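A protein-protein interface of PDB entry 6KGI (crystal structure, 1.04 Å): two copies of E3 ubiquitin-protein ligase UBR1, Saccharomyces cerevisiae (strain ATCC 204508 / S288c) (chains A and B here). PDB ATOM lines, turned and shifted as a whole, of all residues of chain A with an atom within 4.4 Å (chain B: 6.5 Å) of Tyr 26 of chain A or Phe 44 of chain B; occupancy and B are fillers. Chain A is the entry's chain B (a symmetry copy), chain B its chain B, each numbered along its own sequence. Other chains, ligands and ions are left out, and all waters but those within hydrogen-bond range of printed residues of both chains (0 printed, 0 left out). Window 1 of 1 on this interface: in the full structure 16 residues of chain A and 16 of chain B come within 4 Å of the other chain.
The side-chain hydroxyl of Thr 56 of chain A is in hydrogen-bond range of the backbone carbonyl oxygen of Pro 46 of chain B, at 2.9 Å.
OG1 of Thr 56 of chain A sits close to O of His 49 of chain B, at 3.2 Å.
O of Val 54 of chain A lies within hydrogen-bond range of N of Val 54 of chain B.
The backbone NH (N) of Tyr 26 of chain B lies within hydrogen-bond range of the backbone carbonyl oxygen (O) of Leu 39 of chain B (2.9 Å).
N of Tyr 26 of chain A is in hydrogen-bond range of O of Leu 39 of chain A (2.9 Å).
OH of Tyr 26 of chain A touches OH of Tyr 26 of chain B (3.8 Å).
Tyr 26 of chain A touches Phe 44 of chain B (OH to CE2, 3.3 Å).
CG of Pro 46 of chain B touches OH of Tyr 26 of chain A, 3.6 Å away.
Tyr 26 of chain B touches Phe 44 of chain A (OH to CE2, 3.3 Å).
Tyr 26 of chain A touches three residues of chain B.
Phe 44 of chain B touches just one residue of chain A: Tyr 26.
Of the printed residues of chain B, Thr 56 of chain A touches Pro 46 (2.9 Å) and His 49 (3.2 Å).
Printed residues of chain A within 4 Å of His 49 of chain B: Thr 56.
Of the printed residues of chain B, Val 54 of chain A touches Val 54 (3.1 Å).
Printed residues of chain A within 4 Å of Val 54 of chain B: Val 54.
Printed residues of chain A within 4 Å of Tyr 26 of chain B: Tyr 26 (3.8 Å) and Phe 44 (3.3 Å).
The nearest residue of chain B that does not touch Tyr 26 of chain A is Asn 45 of chain B (5.4 Å).
The nearest printed residue of chain A that does not touch Phe 44 of chain B is Thr 56 of chain A (4.4 Å).
Printed residues of chain A that touch a printed residue of chain B: Tyr 26, Phe 44, Val 54 and Thr 56.
Hydrophobic or aromatic side chains of chain A within 4 Å of the printed part of chain B: Tyr 26, Phe 44 and Val 54.
Printed residues of chain B that touch a printed residue of chain A: Tyr 26, Phe 44, Pro 46, His 49 and Val 54.
Hydrophobic or aromatic side chains of chain B that line the printed part of chain A: Tyr 26, Phe 44, Pro 46 and Val 54.
Among the printed residues, 7 pairs touch across the chains.
Tyr 26 of chain B touches its own counterpart, Tyr 26 of chain A.
Tyr 26 of chain A touches Phe 44 of chain B, and with the chains exchanged Phe 44 of chain A touches Tyr 26 of chain B.
Val 54 of chain B touches its own counterpart, Val 54 of chain A.
Positions printed for both chains: 26, 27, 39, 40, 41, 44 and 54.
Of the 7 pairs that touch across the chains among the printed residues, 4 have their exchanged pair printed and touching as well.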
ATOM      1  N   LEU A  25     -24.931  22.092 -15.094  1.00  0.00           N
ATOM      2  CA  LEU A  25     -25.461  21.885 -16.431  1.00  0.00           C
ATOM      3  C   LEU A  25     -24.519  20.936 -17.164  1.00  0.00           C
ATOM      4  O   LEU A  25     -23.434  20.590 -16.669  1.00  0.00           O
ATOM      5  CB  LEU A  25     -25.613  23.217 -17.167  1.00  0.00           C
ATOM      6  CG  LEU A  25     -24.307  23.999 -17.332  1.00  0.00           C
ATOM      7  CD1 LEU A  25     -24.215  24.552 -18.754  1.00  0.00           C
ATOM      8  CD2 LEU A  25     -24.185  25.118 -16.335  1.00  0.00           C
ATOM      9  N   TYR A  26     -24.952  20.521 -18.354  1.00  0.00           N
ATOM     10  CA  TYR A  26     -24.266  19.515 -19.135  1.00  0.00           C
ATOM     11  C   TYR A  26     -23.920  20.023 -20.531  1.00  0.00           C
ATOM     12  O   TYR A  26     -24.680  20.766 -21.164  1.00  0.00           O
ATOM     13  CB  TYR A  26     -25.142  18.270 -19.309  1.00  0.00           C
ATOM     14  CG  TYR A  26     -25.354  17.459 -18.058  1.00  0.00           C
ATOM     15  CD1 TYR A  26     -24.521  16.392 -17.768  1.00  0.00           C
ATOM     16  CD2 TYR A  26     -26.387  17.749 -17.169  1.00  0.00           C
ATOM     17  CE1 TYR A  26     -24.703  15.628 -16.642  1.00  0.00           C
ATOM     18  CE2 TYR A  26     -26.579  16.984 -16.029  1.00  0.00           C
ATOM     19  CZ  TYR A  26     -25.733  15.922 -15.776  1.00  0.00           C
ATOM     20  OH  TYR A  26     -25.876  15.137 -14.648  1.00  0.00           O
ATOM     21  N   ARG A  27     -22.781  19.545 -21.023  1.00  0.00           N
ATOM     22  CA  ARG A  27     -22.354  19.692 -22.403  1.00  0.00           C
ATOM     23  C   ARG A  27     -22.008  18.316 -22.952  1.00  0.00           C
ATOM     24  O   ARG A  27     -21.606  17.423 -22.197  1.00  0.00           O
ATOM     25  CB  ARG A  27     -21.097  20.567 -22.496  1.00  0.00           C
ATOM     26  CG  ARG A  27     -21.211  21.887 -21.749  1.00  0.00           C
ATOM     27  CD  ARG A  27     -19.865  22.652 -21.705  1.00  0.00           C
ATOM     28  NE  ARG A  27     -19.988  23.867 -20.904  1.00  0.00           N
ATOM     29  CZ  ARG A  27     -20.496  25.013 -21.350  1.00  0.00           C
ATOM     30  NH1 ARG A  27     -20.876  25.119 -22.615  1.00  0.00           N
ATOM     31  NH2 ARG A  27     -20.608  26.054 -20.537  1.00  0.00           N
ATOM     32  N   VAL A  38     -25.855  23.773 -24.551  1.00  0.00           N
ATOM     33  CA  VAL A  38     -25.924  23.239 -23.199  1.00  0.00           C
ATOM     34  C   VAL A  38     -27.298  22.668 -22.888  1.00  0.00           C
ATOM     35  O   VAL A  38     -28.314  23.027 -23.501  1.00  0.00           O
ATOM     36  CB  VAL A  38     -25.550  24.301 -22.139  1.00  0.00           C
ATOM     37  CG1 VAL A  38     -24.117  24.761 -22.314  1.00  0.00           C
ATOM     38  CG2 VAL A  38     -26.507  25.487 -22.216  1.00  0.00           C
ATOM     39  N   LEU A  39     -27.312  21.800 -21.875  1.00  0.00           N
ATOM     40  CA  LEU A  39     -28.526  21.161 -21.390  1.00  0.00           C
ATOM     41  C   LEU A  39     -28.617  21.291 -19.876  1.00  0.00           C
ATOM     42  O   LEU A  39     -27.656  20.993 -19.154  1.00  0.00           O
ATOM     43  CB  LEU A  39     -28.543  19.677 -21.751  1.00  0.00           C
ATOM     44  CG  LEU A  39     -28.595  19.376 -23.245  1.00  0.00           C
ATOM     45  CD1 LEU A  39     -28.221  17.933 -23.546  1.00  0.00           C
ATOM     46  CD2 LEU A  39     -29.976  19.696 -23.805  1.00  0.00           C
ATOM     47  N   CYS A  40     -29.786  21.704 -19.395  1.00  0.00           N
ATOM     48  CA  CYS A  40     -30.023  21.777 -17.961  1.00  0.00           C
ATOM     49  C   CYS A  40     -30.174  20.379 -17.379  1.00  0.00           C
ATOM     50  O   CYS A  40     -30.325  19.385 -18.092  1.00  0.00           O
ATOM     51  CB  CYS A  40     -31.244  22.645 -17.664  1.00  0.00           C
ATOM     52  SG  CYS A  40     -32.857  21.843 -17.924  1.00  0.00           S
ATOM     53  N   ILE A  41     -30.116  20.314 -16.047  1.00  0.00           N
ATOM     54  CA  ILE A  41     -30.140  19.023 -15.368  1.00  0.00           C
ATOM     55  C   ILE A  41     -31.471  18.311 -15.567  1.00  0.00           C
ATOM     56  O   ILE A  41     -31.546  17.086 -15.455  1.00  0.00           O
ATOM     57  CB  ILE A  41     -29.812  19.169 -13.867  1.00  0.00           C
ATOM     58  CG1 ILE A  41     -30.852  20.041 -13.156  1.00  0.00           C
ATOM     59  CG2 ILE A  41     -28.408  19.689 -13.687  1.00  0.00           C
ATOM     60  CD1 ILE A  41     -30.612  20.190 -11.672  1.00  0.00           C
ATOM     61  N   PHE A  44     -31.088  16.963 -19.593  1.00  0.00           N
ATOM     62  CA  PHE A  44     -30.028  16.069 -20.028  1.00  0.00           C
ATOM     63  C   PHE A  44     -30.439  14.625 -19.795  1.00  0.00           C
ATOM     64  O   PHE A  44     -30.775  14.238 -18.673  1.00  0.00           O
ATOM     65  CB  PHE A  44     -28.741  16.353 -19.249  1.00  0.00           C
ATOM     66  CG  PHE A  44     -27.615  15.407 -19.593  1.00  0.00           C
ATOM     67  CD1 PHE A  44     -26.816  15.636 -20.706  1.00  0.00           C
ATOM     68  CD2 PHE A  44     -27.375  14.275 -18.832  1.00  0.00           C
ATOM     69  CE1 PHE A  44     -25.794  14.763 -21.049  1.00  0.00           C
ATOM     70  CE2 PHE A  44     -26.354  13.400 -19.171  1.00  0.00           C
ATOM     71  CZ  PHE A  44     -25.563  13.648 -20.286  1.00  0.00           C
ATOM     72  N   VAL A  54     -19.033  13.653 -22.335  1.00  0.00           N
ATOM     73  CA  VAL A  54     -19.887  14.594 -21.627  1.00  0.00           C
ATOM     74  C   VAL A  54     -19.030  15.379 -20.645  1.00  0.00           C
ATOM     75  O   VAL A  54     -18.087  14.850 -20.040  1.00  0.00           O
ATOM     76  CB  VAL A  54     -21.039  13.840 -20.936  1.00  0.00           C
ATOM     77  CG1 VAL A  54     -21.735  14.705 -19.892  1.00  0.00           C
ATOM     78  CG2 VAL A  54     -22.035  13.355 -21.994  1.00  0.00           C
ATOM     79  N   CYS A  55     -19.348  16.664 -20.504  1.00  0.00           N
ATOM     80  CA  CYS A  55     -18.617  17.564 -19.616  1.00  0.00           C
ATOM     81  C   CYS A  55     -19.610  18.439 -18.873  1.00  0.00           C
ATOM     82  O   CYS A  55     -20.338  19.212 -19.506  1.00  0.00           O
ATOM     83  CB  CYS A  55     -17.672  18.451 -20.435  1.00  0.00           C
ATOM     84  SG  CYS A  55     -16.576  19.545 -19.513  1.00  0.00           S
ATOM     85  N   THR A  56     -19.579  18.379 -17.544  1.00  0.00           N
ATOM     86  CA  THR A  56     -20.478  19.203 -16.757  1.00  0.00           C
ATOM     87  C   THR A  56     -19.852  20.570 -16.497  1.00  0.00           C
ATOM     88  O   THR A  56     -18.650  20.790 -16.695  1.00  0.00           O
ATOM     89  CB  THR A  56     -20.854  18.511 -15.441  1.00  0.00           C
ATOM     90  OG1 THR A  56     -19.708  18.488 -14.591  1.00  0.00           O
ATOM     91  CG2 THR A  56     -21.367  17.096 -15.695  1.00  0.00           C
ATOM     92  N   TYR B  26     -23.694   6.313 -14.998  1.00  0.00           N
ATOM     93  CA  TYR B  26     -22.605   7.232 -15.250  1.00  0.00           C
ATOM     94  C   TYR B  26     -21.261   6.642 -14.837  1.00  0.00           C
ATOM     95  O   TYR B  26     -21.139   5.930 -13.833  1.00  0.00           O
ATOM     96  CB  TYR B  26     -22.795   8.529 -14.456  1.00  0.00           C
ATOM     97  CG  TYR B  26     -23.925   9.406 -14.926  1.00  0.00           C
ATOM     98  CD1 TYR B  26     -23.689  10.420 -15.837  1.00  0.00           C
ATOM     99  CD2 TYR B  26     -25.225   9.230 -14.458  1.00  0.00           C
ATOM    100  CE1 TYR B  26     -24.701  11.243 -16.270  1.00  0.00           C
ATOM    101  CE2 TYR B  26     -26.253  10.054 -14.888  1.00  0.00           C
ATOM    102  CZ  TYR B  26     -25.980  11.062 -15.792  1.00  0.00           C
ATOM    103  OH  TYR B  26     -26.971  11.903 -16.260  1.00  0.00           O
ATOM    104  N   ARG B  27     -20.239   7.015 -15.602  1.00  0.00           N
ATOM    105  CA  ARG B  27     -18.842   6.779 -15.283  1.00  0.00           C
ATOM    106  C   ARG B  27     -18.096   8.101 -15.371  1.00  0.00           C
ATOM    107  O   ARG B  27     -18.488   8.994 -16.131  1.00  0.00           O
ATOM    108  CB  ARG B  27     -18.207   5.810 -16.290  1.00  0.00           C
ATOM    109  CG  ARG B  27     -19.008   4.536 -16.507  1.00  0.00           C
ATOM    110  CD  ARG B  27     -18.440   3.678 -17.663  1.00  0.00           C
ATOM    111  NE  ARG B  27     -19.284   2.509 -17.902  1.00  0.00           N
ATOM    112  CZ  ARG B  27     -19.230   1.386 -17.192  1.00  0.00           C
ATOM    113  NH1 ARG B  27     -18.327   1.255 -16.231  1.00  0.00           N
ATOM    114  NH2 ARG B  27     -20.066   0.391 -17.453  1.00  0.00           N
ATOM    115  N   CYS B  28     -17.002   8.216 -14.615  1.00  0.00           N
ATOM    116  CA  CYS B  28     -16.126   9.378 -14.700  1.00  0.00           C
ATOM    117  C   CYS B  28     -14.684   8.899 -14.798  1.00  0.00           C
ATOM    118  O   CYS B  28     -14.194   8.207 -13.901  1.00  0.00           O
ATOM    119  CB  CYS B  28     -16.275  10.312 -13.498  1.00  0.00           C
ATOM    120  SG  CYS B  28     -15.064  11.639 -13.632  1.00  0.00           S
ATOM    121  N   LEU B  39     -21.891   5.062 -11.153  1.00  0.00           N
ATOM    122  CA  LEU B  39     -22.862   5.807 -10.367  1.00  0.00           C
ATOM    123  C   LEU B  39     -24.230   5.748 -11.032  1.00  0.00           C
ATOM    124  O   LEU B  39     -24.363   6.006 -12.236  1.00  0.00           O
ATOM    125  CB  LEU B  39     -22.449   7.272 -10.236  1.00  0.00           C
ATOM    126  CG  LEU B  39     -21.157   7.512  -9.464  1.00  0.00           C
ATOM    127  CD1 LEU B  39     -20.606   8.909  -9.701  1.00  0.00           C
ATOM    128  CD2 LEU B  39     -21.373   7.270  -7.974  1.00  0.00           C
ATOM    129  N   CYS B  40     -25.253   5.442 -10.238  1.00  0.00           N
ATOM    130  CA  CYS B  40     -26.618   5.448 -10.740  1.00  0.00           C
ATOM    131  C   CYS B  40     -27.096   6.876 -10.956  1.00  0.00           C
ATOM    132  O   CYS B  40     -26.479   7.848 -10.514  1.00  0.00           O
ATOM    133  CB  CYS B  40     -27.540   4.684  -9.791  1.00  0.00           C
ATOM    134  SG  CYS B  40     -28.049   5.590  -8.296  1.00  0.00           S
ATOM    135  N   ILE B  41     -28.219   6.993 -11.669  1.00  0.00           N
ATOM    136  CA  ILE B  41     -28.726   8.310 -12.038  1.00  0.00           C
ATOM    137  C   ILE B  41     -29.156   9.108 -10.815  1.00  0.00           C
ATOM    138  O   ILE B  41     -29.200  10.339 -10.858  1.00  0.00           O
ATOM    139  CB  ILE B  41     -29.878   8.204 -13.060  1.00  0.00           C
ATOM    140  CG1 ILE B  41     -31.070   7.441 -12.473  1.00  0.00           C
ATOM    141  CG2 ILE B  41     -29.381   7.592 -14.346  1.00  0.00           C
ATOM    142  CD1 ILE B  41     -32.250   7.338 -13.410  1.00  0.00           C
ATOM    143  N   HIS B  42     -29.553   8.435  -9.731  1.00  0.00           N
ATOM    144  CA  HIS B  42     -30.010   9.125  -8.531  1.00  0.00           C
ATOM    145  C   HIS B  42     -28.857   9.682  -7.723  1.00  0.00           C
ATOM    146  O   HIS B  42     -29.051  10.607  -6.920  1.00  0.00           O
ATOM    147  CB  HIS B  42     -30.850   8.168  -7.695  1.00  0.00           C
ATOM    148  CG  HIS B  42     -31.888   7.475  -8.503  1.00  0.00           C
ATOM    149  ND1 HIS B  42     -32.970   8.140  -9.029  1.00  0.00           N
ATOM    150  CD2 HIS B  42     -31.972   6.200  -8.948  1.00  0.00           C
ATOM    151  CE1 HIS B  42     -33.700   7.292  -9.734  1.00  0.00           C
ATOM    152  NE2 HIS B  42     -33.110   6.112  -9.710  1.00  0.00           N
ATOM    153  N   CYS B  43     -27.664   9.145  -7.929  1.00  0.00           N
ATOM    154  CA  CYS B  43     -26.475   9.499  -7.166  1.00  0.00           C
ATOM    155  C   CYS B  43     -25.541  10.438  -7.905  1.00  0.00           C
ATOM    156  O   CYS B  43     -24.941  11.321  -7.278  1.00  0.00           O
ATOM    157  CB  CYS B  43     -25.700   8.228  -6.814  1.00  0.00           C
ATOM    158  SG  CYS B  43     -26.531   7.239  -5.575  1.00  0.00           S
ATOM    159  N   PHE B  44     -25.376  10.253  -9.211  1.00  0.00           N
ATOM    160  CA  PHE B  44     -24.412  11.048  -9.954  1.00  0.00           C
ATOM    161  C   PHE B  44     -24.711  12.526  -9.773  1.00  0.00           C
ATOM    162  O   PHE B  44     -25.822  12.984 -10.053  1.00  0.00           O
ATOM    163  CB  PHE B  44     -24.476  10.704 -11.444  1.00  0.00           C
ATOM    164  CG  PHE B  44     -23.555  11.551 -12.291  1.00  0.00           C
ATOM    165  CD1 PHE B  44     -22.213  11.217 -12.424  1.00  0.00           C
ATOM    166  CD2 PHE B  44     -24.015  12.693 -12.924  1.00  0.00           C
ATOM    167  CE1 PHE B  44     -21.350  11.998 -13.177  1.00  0.00           C
ATOM    168  CE2 PHE B  44     -23.155  13.476 -13.679  1.00  0.00           C
ATOM    169  CZ  PHE B  44     -21.817  13.125 -13.802  1.00  0.00           C
ATOM    170  N   ASN B  45     -23.703  13.278  -9.340  1.00  0.00           N
ATOM    171  CA  ASN B  45     -23.875  14.700  -9.099  1.00  0.00           C
ATOM    172  C   ASN B  45     -23.006  15.462 -10.081  1.00  0.00           C
ATOM    173  O   ASN B  45     -21.772  15.407  -9.970  1.00  0.00           O
ATOM    174  CB  ASN B  45     -23.484  15.050  -7.663  1.00  0.00           C
ATOM    175  CG  ASN B  45     -23.836  16.472  -7.311  1.00  0.00           C
ATOM    176  OD1 ASN B  45     -24.063  17.304  -8.191  1.00  0.00           O
ATOM    177  ND2 ASN B  45     -23.898  16.767  -6.017  1.00  0.00           N
ATOM    178  N   PRO B  46     -23.584  16.171 -11.052  1.00  0.00           N
ATOM    179  CA  PRO B  46     -22.736  16.887 -12.017  1.00  0.00           C
ATOM    180  C   PRO B  46     -21.793  17.881 -11.364  1.00  0.00           C
ATOM    181  O   PRO B  46     -20.744  18.205 -11.947  1.00  0.00           O
ATOM    182  CB  PRO B  46     -23.750  17.566 -12.953  1.00  0.00           C
ATOM    183  CG  PRO B  46     -25.019  17.634 -12.158  1.00  0.00           C
ATOM    184  CD  PRO B  46     -25.018  16.376 -11.323  1.00  0.00           C
ATOM    185  N   LYS B  47     -22.125  18.370 -10.168  1.00  0.00           N
ATOM    186  CA  LYS B  47     -21.254  19.322  -9.498  1.00  0.00           C
ATOM    187  C   LYS B  47     -19.918  18.708  -9.103  1.00  0.00           C
ATOM    188  O   LYS B  47     -18.973  19.454  -8.825  1.00  0.00           O
ATOM    189  CB  LYS B  47     -21.917  19.864  -8.234  1.00  0.00           C
ATOM    190  CG  LYS B  47     -23.168  20.671  -8.458  1.00  0.00           C
ATOM    191  CD  LYS B  47     -23.810  21.027  -7.129  1.00  0.00           C
ATOM    192  CE  LYS B  47     -25.153  21.684  -7.304  1.00  0.00           C
ATOM    193  NZ  LYS B  47     -25.893  21.748  -6.012  1.00  0.00           N
ATOM    194  N   ASP B  48     -19.815  17.381  -9.042  1.00  0.00           N
ATOM    195  CA  ASP B  48     -18.567  16.733  -8.659  1.00  0.00           C
ATOM    196  C   ASP B  48     -17.587  16.588  -9.816  1.00  0.00           C
ATOM    197  O   ASP B  48     -16.448  16.160  -9.590  1.00  0.00           O
ATOM    198  CB  ASP B  48     -18.847  15.313  -8.129  1.00  0.00           C
ATOM    199  CG  ASP B  48     -19.427  15.285  -6.723  1.00  0.00           C
ATOM    200  OD1 ASP B  48     -19.071  16.170  -5.904  1.00  0.00           O
ATOM    201  OD2 ASP B  48     -20.190  14.330  -6.419  1.00  0.00           O
ATOM    202  N   HIS B  49     -17.996  16.911 -11.043  1.00  0.00           N
ATOM    203  CA  HIS B  49     -17.255  16.444 -12.211  1.00  0.00           C
ATOM    204  C   HIS B  49     -17.003  17.519 -13.259  1.00  0.00           C
ATOM    205  O   HIS B  49     -16.771  17.181 -14.421  1.00  0.00           O
ATOM    206  CB  HIS B  49     -17.967  15.244 -12.836  1.00  0.00           C
ATOM    207  CG  HIS B  49     -18.258  14.163 -11.855  1.00  0.00           C
ATOM    208  ND1 HIS B  49     -17.278  13.342 -11.346  1.00  0.00           N
ATOM    209  CD2 HIS B  49     -19.414  13.804 -11.247  1.00  0.00           C
ATOM    210  CE1 HIS B  49     -17.822  12.510 -10.473  1.00  0.00           C
ATOM    211  NE2 HIS B  49     -19.118  12.769 -10.395  1.00  0.00           N
ATOM    212  N   VAL B  54     -16.829  12.557 -18.455  1.00  0.00           N
ATOM    213  CA  VAL B  54     -17.932  11.711 -18.024  1.00  0.00           C
ATOM    214  C   VAL B  54     -18.420  10.908 -19.221  1.00  0.00           C
ATOM    215  O   VAL B  54     -18.443  11.393 -20.361  1.00  0.00           O
ATOM    216  CB  VAL B  54     -19.043  12.576 -17.399  1.00  0.00           C
ATOM    217  CG1 VAL B  54     -20.354  11.809 -17.275  1.00  0.00           C
ATOM    218  CG2 VAL B  54     -18.579  13.087 -16.031  1.00  0.00           C
ATOM    219  N   CYS B  67     -24.480   0.261  -8.119  1.00  0.00           N
ATOM    220  CA  CYS B  67     -23.945   1.606  -7.948  1.00  0.00           C
ATOM    221  C   CYS B  67     -22.930   1.645  -6.812  1.00  0.00           C
ATOM    222  O   CYS B  67     -23.191   1.132  -5.713  1.00  0.00           O
ATOM    223  CB  CYS B  67     -25.086   2.557  -7.608  1.00  0.00           C
ATOM    224  SG  CYS B  67     -24.571   4.241  -7.275  1.00  0.00           S
ATOM    225  N   CYS B  69     -21.739   4.532  -5.413  1.00  0.00           N
ATOM    226  CA  CYS B  69     -21.783   5.753  -4.619  1.00  0.00           C
ATOM    227  C   CYS B  69     -21.689   5.398  -3.137  1.00  0.00           C
ATOM    228  O   CYS B  69     -22.373   4.490  -2.669  1.00  0.00           O
ATOM    229  CB  CYS B  69     -23.082   6.505  -4.905  1.00  0.00           C
ATOM    230  SG  CYS B  69     -23.112   8.179  -4.179  1.00  0.00           S
ATOM    231  N   HIS B  80     -20.398  13.838  -3.630  1.00  0.00           N
ATOM    232  CA  HIS B  80     -21.486  14.464  -2.876  1.00  0.00           C
ATOM    233  C   HIS B  80     -22.768  13.975  -3.525  1.00  0.00           C
ATOM    234  O   HIS B  80     -23.227  14.532  -4.524  1.00  0.00           O
ATOM    235  CB  HIS B  80     -21.324  15.962  -2.894  1.00  0.00           C
ATOM    236  CG  HIS B  80     -19.985  16.394  -2.396  1.00  0.00           C
ATOM    237  ND1 HIS B  80     -18.871  16.401  -3.205  1.00  0.00           N
ATOM    238  CD2 HIS B  80     -19.558  16.766  -1.163  1.00  0.00           C
ATOM    239  CE1 HIS B  80     -17.821  16.784  -2.503  1.00  0.00           C
ATOM    240  NE2 HIS B  80     -18.209  17.012  -1.261  1.00  0.00           N
ATOM    241  N   CYS B  81     -23.326  12.908  -2.960  1.00  0.00           N
ATOM    242  CA  CYS B  81     -24.444  12.218  -3.584  1.00  0.00           C
ATOM    243  C   CYS B  81     -25.568  13.190  -3.916  1.00  0.00           C
ATOM    244  O   CYS B  81     -26.014  13.964  -3.063  1.00  0.00           O
ATOM    245  CB  CYS B  81     -24.957  11.131  -2.643  1.00  0.00           C
ATOM    246  SG  CYS B  81     -26.356  10.214  -3.325  1.00  0.00           S
ATOM    247  N   LYS B  82     -26.059  13.116  -5.155  1.00  0.00           N
ATOM    248  CA  LYS B  82     -27.141  14.006  -5.554  1.00  0.00           C
ATOM    249  C   LYS B  82     -28.374  13.804  -4.685  1.00  0.00           C
ATOM    250  O   LYS B  82     -29.106  14.761  -4.402  1.00  0.00           O
ATOM    251  CB  LYS B  82     -27.479  13.790  -7.023  1.00  0.00           C
ATOM    252  CG  LYS B  82     -28.447  14.836  -7.562  1.00  0.00           C
ATOM    253  CD  LYS B  82     -28.720  14.645  -9.033  1.00  0.00           C
ATOM    254  CE  LYS B  82     -29.583  13.419  -9.244  1.00  0.00           C
ATOM    255  NZ  LYS B  82     -30.102  13.378 -10.634  1.00  0.00           N
ATOM    256  N   ALA B  83     -28.621  12.572  -4.243  1.00  0.00           N
ATOM    257  CA  ALA B  83     -29.810  12.273  -3.451  1.00  0.00           C
ATOM    258  C   ALA B  83     -29.748  12.842  -2.043  1.00  0.00           C
ATOM    259  O   ALA B  83     -30.775  12.860  -1.356  1.00  0.00           O
ATOM    260  CB  ALA B  83     -30.026  10.764  -3.383  1.00  0.00           C
